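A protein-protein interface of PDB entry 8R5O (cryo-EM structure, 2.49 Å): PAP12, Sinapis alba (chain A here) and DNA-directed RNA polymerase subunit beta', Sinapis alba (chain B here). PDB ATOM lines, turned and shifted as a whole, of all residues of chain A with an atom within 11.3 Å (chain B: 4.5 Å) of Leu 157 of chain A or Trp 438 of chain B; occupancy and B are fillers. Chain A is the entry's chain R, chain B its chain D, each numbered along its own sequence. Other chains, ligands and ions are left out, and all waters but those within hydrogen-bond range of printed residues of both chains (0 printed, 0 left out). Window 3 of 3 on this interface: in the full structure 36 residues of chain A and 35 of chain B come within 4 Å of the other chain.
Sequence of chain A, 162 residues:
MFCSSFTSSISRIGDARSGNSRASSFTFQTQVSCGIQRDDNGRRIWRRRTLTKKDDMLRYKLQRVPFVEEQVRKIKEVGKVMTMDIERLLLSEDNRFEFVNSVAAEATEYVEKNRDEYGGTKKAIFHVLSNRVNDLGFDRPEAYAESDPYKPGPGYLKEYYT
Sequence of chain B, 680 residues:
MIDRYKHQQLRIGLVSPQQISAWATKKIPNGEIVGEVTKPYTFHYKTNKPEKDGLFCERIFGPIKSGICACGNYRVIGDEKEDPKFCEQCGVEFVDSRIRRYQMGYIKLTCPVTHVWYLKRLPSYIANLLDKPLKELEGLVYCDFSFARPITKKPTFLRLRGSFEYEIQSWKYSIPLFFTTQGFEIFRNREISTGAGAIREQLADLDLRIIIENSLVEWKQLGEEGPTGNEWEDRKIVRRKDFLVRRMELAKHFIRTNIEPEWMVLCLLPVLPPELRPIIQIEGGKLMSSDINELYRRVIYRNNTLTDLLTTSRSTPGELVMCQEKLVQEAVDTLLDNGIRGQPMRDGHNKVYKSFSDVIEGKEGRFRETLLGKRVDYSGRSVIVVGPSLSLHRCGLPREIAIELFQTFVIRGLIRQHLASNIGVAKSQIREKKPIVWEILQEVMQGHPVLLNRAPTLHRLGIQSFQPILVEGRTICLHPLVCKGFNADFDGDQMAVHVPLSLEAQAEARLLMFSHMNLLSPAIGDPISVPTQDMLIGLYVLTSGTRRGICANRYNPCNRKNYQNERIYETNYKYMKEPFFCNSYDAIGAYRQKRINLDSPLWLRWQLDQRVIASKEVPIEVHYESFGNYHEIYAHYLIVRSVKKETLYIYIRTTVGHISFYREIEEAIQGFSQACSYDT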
ATOM      1  N   GLY A 120      16.090  30.416 -16.460  1.00  0.00           N
ATOM      2  CA  GLY A 120      15.310  29.220 -16.214  1.00  0.00           C
ATOM      3  C   GLY A 120      13.930  29.512 -15.662  1.00  0.00           C
ATOM      4  O   GLY A 120      13.040  29.955 -16.393  1.00  0.00           O
ATOM      5  N   THR A 121      13.742  29.265 -14.365  1.00  0.00           N
ATOM      6  CA  THR A 121      12.455  29.528 -13.732  1.00  0.00           C
ATOM      7  C   THR A 121      12.217  31.018 -13.528  1.00  0.00           C
ATOM      8  O   THR A 121      11.065  31.466 -13.546  1.00  0.00           O
ATOM      9  CB  THR A 121      12.369  28.794 -12.394  1.00  0.00           C
ATOM     10  OG1 THR A 121      12.871  27.459 -12.545  1.00  0.00           O
ATOM     11  CG2 THR A 121      10.927  28.725 -11.912  1.00  0.00           C
ATOM     12  N   ASP A 148       4.001  23.525 -10.137  1.00  0.00           N
ATOM     13  CA  ASP A 148       2.946  22.557  -9.860  1.00  0.00           C
ATOM     14  C   ASP A 148       3.264  21.807  -8.573  1.00  0.00           C
ATOM     15  O   ASP A 148       4.313  21.157  -8.490  1.00  0.00           O
ATOM     16  CB  ASP A 148       2.804  21.583 -11.024  1.00  0.00           C
ATOM     17  CG  ASP A 148       1.574  20.698 -10.905  1.00  0.00           C
ATOM     18  OD1 ASP A 148       1.486  19.912  -9.940  1.00  0.00           O
ATOM     19  OD2 ASP A 148       0.689  20.794 -11.781  1.00  0.00           O
ATOM     20  N   TYR A 150       1.584  19.213  -7.409  1.00  0.00           N
ATOM     21  CA  TYR A 150       1.117  17.838  -7.511  1.00  0.00           C
ATOM     22  C   TYR A 150       1.971  17.001  -8.456  1.00  0.00           C
ATOM     23  O   TYR A 150       1.498  15.987  -8.976  1.00  0.00           O
ATOM     24  CB  TYR A 150      -0.345  17.815  -7.956  1.00  0.00           C
ATOM     25  CG  TYR A 150      -1.189  18.890  -7.312  1.00  0.00           C
ATOM     26  CD1 TYR A 150      -1.606  18.779  -5.993  1.00  0.00           C
ATOM     27  CD2 TYR A 150      -1.565  20.021  -8.024  1.00  0.00           C
ATOM     28  CE1 TYR A 150      -2.374  19.764  -5.403  1.00  0.00           C
ATOM     29  CE2 TYR A 150      -2.334  21.007  -7.444  1.00  0.00           C
ATOM     30  CZ  TYR A 150      -2.735  20.875  -6.132  1.00  0.00           C
ATOM     31  OH  TYR A 150      -3.501  21.859  -5.552  1.00  0.00           O
ATOM     32  N   LYS A 151       3.213  17.407  -8.689  1.00  0.00           N
ATOM     33  CA  LYS A 151       4.097  16.644  -9.560  1.00  0.00           C
ATOM     34  C   LYS A 151       4.546  15.374  -8.848  1.00  0.00           C
ATOM     35  O   LYS A 151       5.069  15.448  -7.730  1.00  0.00           O
ATOM     36  CB  LYS A 151       5.304  17.489  -9.958  1.00  0.00           C
ATOM     37  CG  LYS A 151       6.169  16.871 -11.041  1.00  0.00           C
ATOM     38  CD  LYS A 151       7.473  17.636 -11.239  1.00  0.00           C
ATOM     39  CE  LYS A 151       7.236  19.077 -11.671  1.00  0.00           C
ATOM     40  NZ  LYS A 151       7.161  20.025 -10.523  1.00  0.00           N
ATOM     41  N   PRO A 152       4.366  14.197  -9.450  1.00  0.00           N
ATOM     42  CA  PRO A 152       4.668  12.924  -8.781  1.00  0.00           C
ATOM     43  C   PRO A 152       6.155  12.571  -8.746  1.00  0.00           C
ATOM     44  O   PRO A 152       6.552  11.446  -9.054  1.00  0.00           O
ATOM     45  CB  PRO A 152       3.867  11.914  -9.607  1.00  0.00           C
ATOM     46  CG  PRO A 152       3.849  12.497 -10.968  1.00  0.00           C
ATOM     47  CD  PRO A 152       3.785  13.991 -10.788  1.00  0.00           C
ATOM     48  N   GLY A 153       6.983  13.536  -8.356  1.00  0.00           N
ATOM     49  CA  GLY A 153       8.399  13.305  -8.198  1.00  0.00           C
ATOM     50  C   GLY A 153       9.216  13.708  -9.409  1.00  0.00           C
ATOM     51  O   GLY A 153       8.684  14.169 -10.424  1.00  0.00           O
ATOM     52  N   PRO A 154      10.531  13.540  -9.318  1.00  0.00           N
ATOM     53  CA  PRO A 154      11.408  13.937 -10.423  1.00  0.00           C
ATOM     54  C   PRO A 154      11.220  13.052 -11.646  1.00  0.00           C
ATOM     55  O   PRO A 154      10.809  11.892 -11.559  1.00  0.00           O
ATOM     56  CB  PRO A 154      12.814  13.777  -9.836  1.00  0.00           C
ATOM     57  CG  PRO A 154      12.654  12.747  -8.774  1.00  0.00           C
ATOM     58  CD  PRO A 154      11.287  12.969  -8.190  1.00  0.00           C
ATOM     59  N   GLY A 155      11.531  13.629 -12.805  1.00  0.00           N
ATOM     60  CA  GLY A 155      11.414  12.945 -14.070  1.00  0.00           C
ATOM     61  C   GLY A 155      10.064  13.072 -14.742  1.00  0.00           C
ATOM     62  O   GLY A 155       9.956  12.795 -15.941  1.00  0.00           O
ATOM     63  N   TYR A 156       9.036  13.495 -14.011  1.00  0.00           N
ATOM     64  CA  TYR A 156       7.680  13.561 -14.540  1.00  0.00           C
ATOM     65  C   TYR A 156       7.407  14.955 -15.088  1.00  0.00           C
ATOM     66  O   TYR A 156       7.585  15.953 -14.383  1.00  0.00           O
ATOM     67  CB  TYR A 156       6.662  13.206 -13.459  1.00  0.00           C
ATOM     68  CG  TYR A 156       6.511  11.723 -13.225  1.00  0.00           C
ATOM     69  CD1 TYR A 156       5.591  10.980 -13.948  1.00  0.00           C
ATOM     70  CD2 TYR A 156       7.286  11.066 -12.280  1.00  0.00           C
ATOM     71  CE1 TYR A 156       5.446   9.626 -13.739  1.00  0.00           C
ATOM     72  CE2 TYR A 156       7.148   9.709 -12.063  1.00  0.00           C
ATOM     73  CZ  TYR A 156       6.225   8.994 -12.797  1.00  0.00           C
ATOM     74  OH  TYR A 156       6.079   7.643 -12.591  1.00  0.00           O
ATOM     75  N   LEU A 157       6.975  15.018 -16.342  1.00  0.00           N
ATOM     76  CA  LEU A 157       6.550  16.262 -16.968  1.00  0.00           C
ATOM     77  C   LEU A 157       5.033  16.283 -17.063  1.00  0.00           C
ATOM     78  O   LEU A 157       4.423  15.298 -17.490  1.00  0.00           O
ATOM     79  CB  LEU A 157       7.150  16.416 -18.365  1.00  0.00           C
ATOM     80  CG  LEU A 157       8.663  16.527 -18.523  1.00  0.00           C
ATOM     81  CD1 LEU A 157       8.979  16.886 -19.957  1.00  0.00           C
ATOM     82  CD2 LEU A 157       9.231  17.561 -17.577  1.00  0.00           C
ATOM     83  N   LYS A 158       4.430  17.399 -16.665  1.00  0.00           N
ATOM     84  CA  LYS A 158       3.010  17.584 -16.915  1.00  0.00           C
ATOM     85  C   LYS A 158       2.764  17.634 -18.417  1.00  0.00           C
ATOM     86  O   LYS A 158       3.470  18.329 -19.152  1.00  0.00           O
ATOM     87  CB  LYS A 158       2.511  18.864 -16.246  1.00  0.00           C
ATOM     88  CG  LYS A 158       1.002  19.007 -16.255  1.00  0.00           C
ATOM     89  CD  LYS A 158       0.559  20.270 -15.544  1.00  0.00           C
ATOM     90  CE  LYS A 158      -0.952  20.402 -15.564  1.00  0.00           C
ATOM     91  NZ  LYS A 158      -1.490  20.373 -16.951  1.00  0.00           N
ATOM     92  N   GLU A 159       1.761  16.893 -18.872  1.00  0.00           N
ATOM     93  CA  GLU A 159       1.482  16.732 -20.291  1.00  0.00           C
ATOM     94  C   GLU A 159       0.235  17.520 -20.656  1.00  0.00           C
ATOM     95  O   GLU A 159      -0.799  17.396 -19.992  1.00  0.00           O
ATOM     96  CB  GLU A 159       1.309  15.256 -20.647  1.00  0.00           C
ATOM     97  CG  GLU A 159       2.519  14.404 -20.308  1.00  0.00           C
ATOM     98  CD  GLU A 159       2.260  12.921 -20.481  1.00  0.00           C
ATOM     99  OE1 GLU A 159       1.086  12.539 -20.659  1.00  0.00           O
ATOM    100  OE2 GLU A 159       3.232  12.140 -20.442  1.00  0.00           O
ATOM    101  N   TYR A 160       0.335  18.324 -21.708  1.00  0.00           N
ATOM    102  CA  TYR A 160      -0.771  19.169 -22.131  1.00  0.00           C
ATOM    103  C   TYR A 160      -1.636  18.468 -23.171  1.00  0.00           C
ATOM    104  O   TYR A 160      -1.140  18.025 -24.206  1.00  0.00           O
ATOM    105  CB  TYR A 160      -0.244  20.492 -22.687  1.00  0.00           C
ATOM    106  CG  TYR A 160      -1.302  21.560 -22.813  1.00  0.00           C
ATOM    107  CD1 TYR A 160      -1.617  22.378 -21.737  1.00  0.00           C
ATOM    108  CD2 TYR A 160      -1.988  21.752 -24.004  1.00  0.00           C
ATOM    109  CE1 TYR A 160      -2.583  23.355 -21.843  1.00  0.00           C
ATOM    110  CE2 TYR A 160      -2.956  22.729 -24.120  1.00  0.00           C
ATOM    111  CZ  TYR A 160      -3.249  23.527 -23.035  1.00  0.00           C
ATOM    112  OH  TYR A 160      -4.211  24.502 -23.138  1.00  0.00           O
ATOM    113  N   ARG B 399       8.040  18.655 -29.123  1.00  0.00           N
ATOM    114  CA  ARG B 399       9.377  18.497 -28.556  1.00  0.00           C
ATOM    115  C   ARG B 399      10.451  18.598 -29.630  1.00  0.00           C
ATOM    116  O   ARG B 399      11.495  19.224 -29.416  1.00  0.00           O
ATOM    117  CB  ARG B 399       9.494  17.158 -27.833  1.00  0.00           C
ATOM    118  CG  ARG B 399       8.885  17.117 -26.453  1.00  0.00           C
ATOM    119  CD  ARG B 399       9.218  15.801 -25.780  1.00  0.00           C
ATOM    120  NE  ARG B 399       8.705  15.727 -24.419  1.00  0.00           N
ATOM    121  CZ  ARG B 399       8.895  14.697 -23.607  1.00  0.00           C
ATOM    122  NH1 ARG B 399       9.588  13.636 -23.987  1.00  0.00           N
ATOM    123  NH2 ARG B 399       8.376  14.731 -22.383  1.00  0.00           N
ATOM    124  N   ILE B 403      13.030  21.714 -29.130  1.00  0.00           N
ATOM    125  CA  ILE B 403      14.406  21.461 -28.716  1.00  0.00           C
ATOM    126  C   ILE B 403      15.390  22.090 -29.695  1.00  0.00           C
ATOM    127  O   ILE B 403      16.464  22.550 -29.291  1.00  0.00           O
ATOM    128  CB  ILE B 403      14.652  19.950 -28.536  1.00  0.00           C
ATOM    129  CG1 ILE B 403      15.959  19.715 -27.784  1.00  0.00           C
ATOM    130  CG2 ILE B 403      14.676  19.223 -29.870  1.00  0.00           C
ATOM    131  CD1 ILE B 403      15.983  20.328 -26.408  1.00  0.00           C
ATOM    132  N   LYS B 433      18.714  12.020 -26.076  1.00  0.00           N
ATOM    133  CA  LYS B 433      17.372  12.143 -25.504  1.00  0.00           C
ATOM    134  C   LYS B 433      17.353  11.770 -24.023  1.00  0.00           C
ATOM    135  O   LYS B 433      16.432  11.107 -23.546  1.00  0.00           O
ATOM    136  CB  LYS B 433      16.355  11.304 -26.282  1.00  0.00           C
ATOM    137  CG  LYS B 433      16.230  11.648 -27.755  1.00  0.00           C
ATOM    138  CD  LYS B 433      15.812  13.094 -27.959  1.00  0.00           C
ATOM    139  CE  LYS B 433      15.051  13.265 -29.266  1.00  0.00           C
ATOM    140  NZ  LYS B 433      15.768  12.664 -30.425  1.00  0.00           N
ATOM    141  N   LYS B 434      18.382  12.190 -23.296  1.00  0.00           N
ATOM    142  CA  LYS B 434      18.402  11.983 -21.856  1.00  0.00           C
ATOM    143  C   LYS B 434      17.205  12.698 -21.235  1.00  0.00           C
ATOM    144  O   LYS B 434      16.970  13.876 -21.538  1.00  0.00           O
ATOM    145  CB  LYS B 434      19.711  12.500 -21.259  1.00  0.00           C
ATOM    146  CG  LYS B 434      19.935  12.149 -19.794  1.00  0.00           C
ATOM    147  CD  LYS B 434      20.120  10.651 -19.593  1.00  0.00           C
ATOM    148  CE  LYS B 434      21.273  10.106 -20.422  1.00  0.00           C
ATOM    149  NZ  LYS B 434      22.576  10.725 -20.059  1.00  0.00           N
ATOM    150  N   PRO B 435      16.423  12.029 -20.382  1.00  0.00           N
ATOM    151  CA  PRO B 435      15.157  12.627 -19.920  1.00  0.00           C
ATOM    152  C   PRO B 435      15.324  13.940 -19.176  1.00  0.00           C
ATOM    153  O   PRO B 435      14.358  14.710 -19.094  1.00  0.00           O
ATOM    154  CB  PRO B 435      14.572  11.540 -19.007  1.00  0.00           C
ATOM    155  CG  PRO B 435      15.187  10.272 -19.494  1.00  0.00           C
ATOM    156  CD  PRO B 435      16.575  10.638 -19.926  1.00  0.00           C
ATOM    157  N   ILE B 436      16.508  14.224 -18.631  1.00  0.00           N
ATOM    158  CA  ILE B 436      16.737  15.494 -17.953  1.00  0.00           C
ATOM    159  C   ILE B 436      16.683  16.664 -18.927  1.00  0.00           C
ATOM    160  O   ILE B 436      16.480  17.809 -18.510  1.00  0.00           O
ATOM    161  CB  ILE B 436      18.084  15.449 -17.199  1.00  0.00           C
ATOM    162  CG1 ILE B 436      18.179  16.595 -16.191  1.00  0.00           C
ATOM    163  CG2 ILE B 436      19.250  15.489 -18.176  1.00  0.00           C
ATOM    164  CD1 ILE B 436      17.078  16.593 -15.158  1.00  0.00           C
ATOM    165  N   VAL B 437      16.853  16.402 -20.225  1.00  0.00           N
ATOM    166  CA  VAL B 437      16.798  17.468 -21.223  1.00  0.00           C
ATOM    167  C   VAL B 437      15.409  18.093 -21.267  1.00  0.00           C
ATOM    168  O   VAL B 437      15.265  19.317 -21.354  1.00  0.00           O
ATOM    169  CB  VAL B 437      17.219  16.926 -22.603  1.00  0.00           C
ATOM    170  CG1 VAL B 437      16.970  17.961 -23.685  1.00  0.00           C
ATOM    171  CG2 VAL B 437      18.680  16.514 -22.581  1.00  0.00           C
ATOM    172  N   TRP B 438      14.366  17.264 -21.205  1.00  0.00           N
ATOM    173  CA  TRP B 438      13.008  17.774 -21.346  1.00  0.00           C
ATOM    174  C   TRP B 438      12.571  18.579 -20.129  1.00  0.00           C
ATOM    175  O   TRP B 438      11.766  19.506 -20.261  1.00  0.00           O
ATOM    176  CB  TRP B 438      12.043  16.622 -21.611  1.00  0.00           C
ATOM    177  CG  TRP B 438      12.469  15.747 -22.747  1.00  0.00           C
ATOM    178  CD1 TRP B 438      12.769  14.420 -22.688  1.00  0.00           C
ATOM    179  CD2 TRP B 438      12.662  16.142 -24.111  1.00  0.00           C
ATOM    180  NE1 TRP B 438      13.126  13.959 -23.932  1.00  0.00           N
ATOM    181  CE2 TRP B 438      13.068  14.999 -24.823  1.00  0.00           C
ATOM    182  CE3 TRP B 438      12.522  17.351 -24.799  1.00  0.00           C
ATOM    183  CZ2 TRP B 438      13.339  15.028 -26.189  1.00  0.00           C
ATOM    184  CZ3 TRP B 438      12.792  17.378 -26.154  1.00  0.00           C
ATOM    185  CH2 TRP B 438      13.195  16.224 -26.834  1.00  0.00           C
ATOM    186  N   GLU B 439      13.078  18.241 -18.941  1.00  0.00           N
ATOM    187  CA  GLU B 439      12.821  19.072 -17.769  1.00  0.00           C
ATOM    188  C   GLU B 439      13.421  20.462 -17.940  1.00  0.00           C
ATOM    189  O   GLU B 439      12.786  21.467 -17.605  1.00  0.00           O
ATOM    190  CB  GLU B 439      13.377  18.400 -16.514  1.00  0.00           C
ATOM    191  CG  GLU B 439      12.375  17.546 -15.759  1.00  0.00           C
ATOM    192  CD  GLU B 439      11.376  18.376 -14.973  1.00  0.00           C
ATOM    193  OE1 GLU B 439      11.619  19.587 -14.790  1.00  0.00           O
ATOM    194  OE2 GLU B 439      10.348  17.815 -14.538  1.00  0.00           O
ATOM    195  N   ILE B 440      14.646  20.536 -18.463  1.00  0.00           N
ATOM    196  CA  ILE B 440      15.283  21.828 -18.702  1.00  0.00           C
ATOM    197  C   ILE B 440      14.552  22.589 -19.799  1.00  0.00           C
ATOM    198  O   ILE B 440      14.379  23.811 -19.715  1.00  0.00           O
ATOM    199  CB  ILE B 440      16.773  21.631 -19.041  1.00  0.00           C
ATOM    200  CG1 ILE B 440      17.509  20.988 -17.865  1.00  0.00           C
ATOM    201  CG2 ILE B 440      17.420  22.955 -19.412  1.00  0.00           C
ATOM    202  CD1 ILE B 440      17.546  21.848 -16.627  1.00  0.00           C
ATOM    203  N   LEU B 441      14.111  21.884 -20.844  1.00  0.00           N
ATOM    204  CA  LEU B 441      13.430  22.544 -21.954  1.00  0.00           C
ATOM    205  C   LEU B 441      12.163  23.249 -21.487  1.00  0.00           C
ATOM    206  O   LEU B 441      11.863  24.362 -21.935  1.00  0.00           O
ATOM    207  CB  LEU B 441      13.111  21.529 -23.052  1.00  0.00           C
ATOM    208  CG  LEU B 441      12.399  22.069 -24.294  1.00  0.00           C
ATOM    209  CD1 LEU B 441      13.213  23.167 -24.953  1.00  0.00           C
ATOM    210  CD2 LEU B 441      12.108  20.952 -25.282  1.00  0.00           C
ATOM    211  N   GLN B 442      11.408  22.623 -20.581  1.00  0.00           N
ATOM    212  CA  GLN B 442      10.220  23.274 -20.038  1.00  0.00           C
ATOM    213  C   GLN B 442      10.580  24.534 -19.262  1.00  0.00           C
ATOM    214  O   GLN B 442       9.862  25.538 -19.328  1.00  0.00           O
ATOM    215  CB  GLN B 442       9.443  22.307 -19.146  1.00  0.00           C
ATOM    216  CG  GLN B 442       8.332  21.559 -19.858  1.00  0.00           C
ATOM    217  CD  GLN B 442       7.344  20.931 -18.894  1.00  0.00           C
ATOM    218  OE1 GLN B 442       7.481  21.056 -17.677  1.00  0.00           O
ATOM    219  NE2 GLN B 442       6.338  20.253 -19.435  1.00  0.00           N
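CD1 of Leu 157 of chain A touches NH2 of Arg 399 of chain B, at 3.3 Å.
Leu 157 of chain A touches Trp 438 of chain B.
Leu 157 of chain A touches Glu 439 of chain B.
CD2 of Leu 157 of chain A touches OE1 of Gln 442 of chain B (3.9 Å).
O of Lys 158 of chain A is in hydrogen-bond range of NE2 of Gln 442 of chain B (3.5 Å).
O of Tyr 156 of chain A sits close to OE2 of Glu 439 of chain B (3.3 Å).
Of chain B, only Arg 399 (3.3 Å), Trp 438 (3.5 Å), Glu 439 (3.2 Å) and Gln 442 (3.9 Å) come within 4 Å of Leu 157 of chain A.
Of the printed residues of chain A, Arg 399 of chain B touches Leu 157.
No residue of chain A comes within 4 Å of Lys 433 of chain B.
No residue of chain A comes within 4 Å of Pro 435 of chain B.
No residue of chain A comes within 4 Å of Ile 436 of chain B.
Of chain A, only Tyr 156 and Leu 157 come within 4 Å of Glu 439 of chain B.
No residue of chain A comes within 4 Å of Leu 441 of chain B.
Of the printed residues of chain B, Tyr 156 of chain A touches Glu 439 (3.3 Å).
Of the printed residues of chain B, Lys 158 of chain A touches Gln 442 (3.5 Å).
The nearest printed residue of chain B that does not touch Lys 158 of chain A is Glu 439 of chain B (6.3 Å).
Printed residues of chain A that touch a printed residue of chain B: Tyr 156, Leu 157 and Lys 158.
Hydrophobic or aromatic side chains of chain A within 4 Å of the printed part of chain B: Leu 157.
Along chain A the printed residues that touch a printed residue of chain B span positions 156 to 158.
Hydrophobic or aromatic side chains of chain B within 4 Å of the printed part of chain A: Trp 438.
Among the printed residues, no Asp or Glu carboxylate lies within 4 Å of a Lys or Arg side-chain nitrogen of the other chain.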
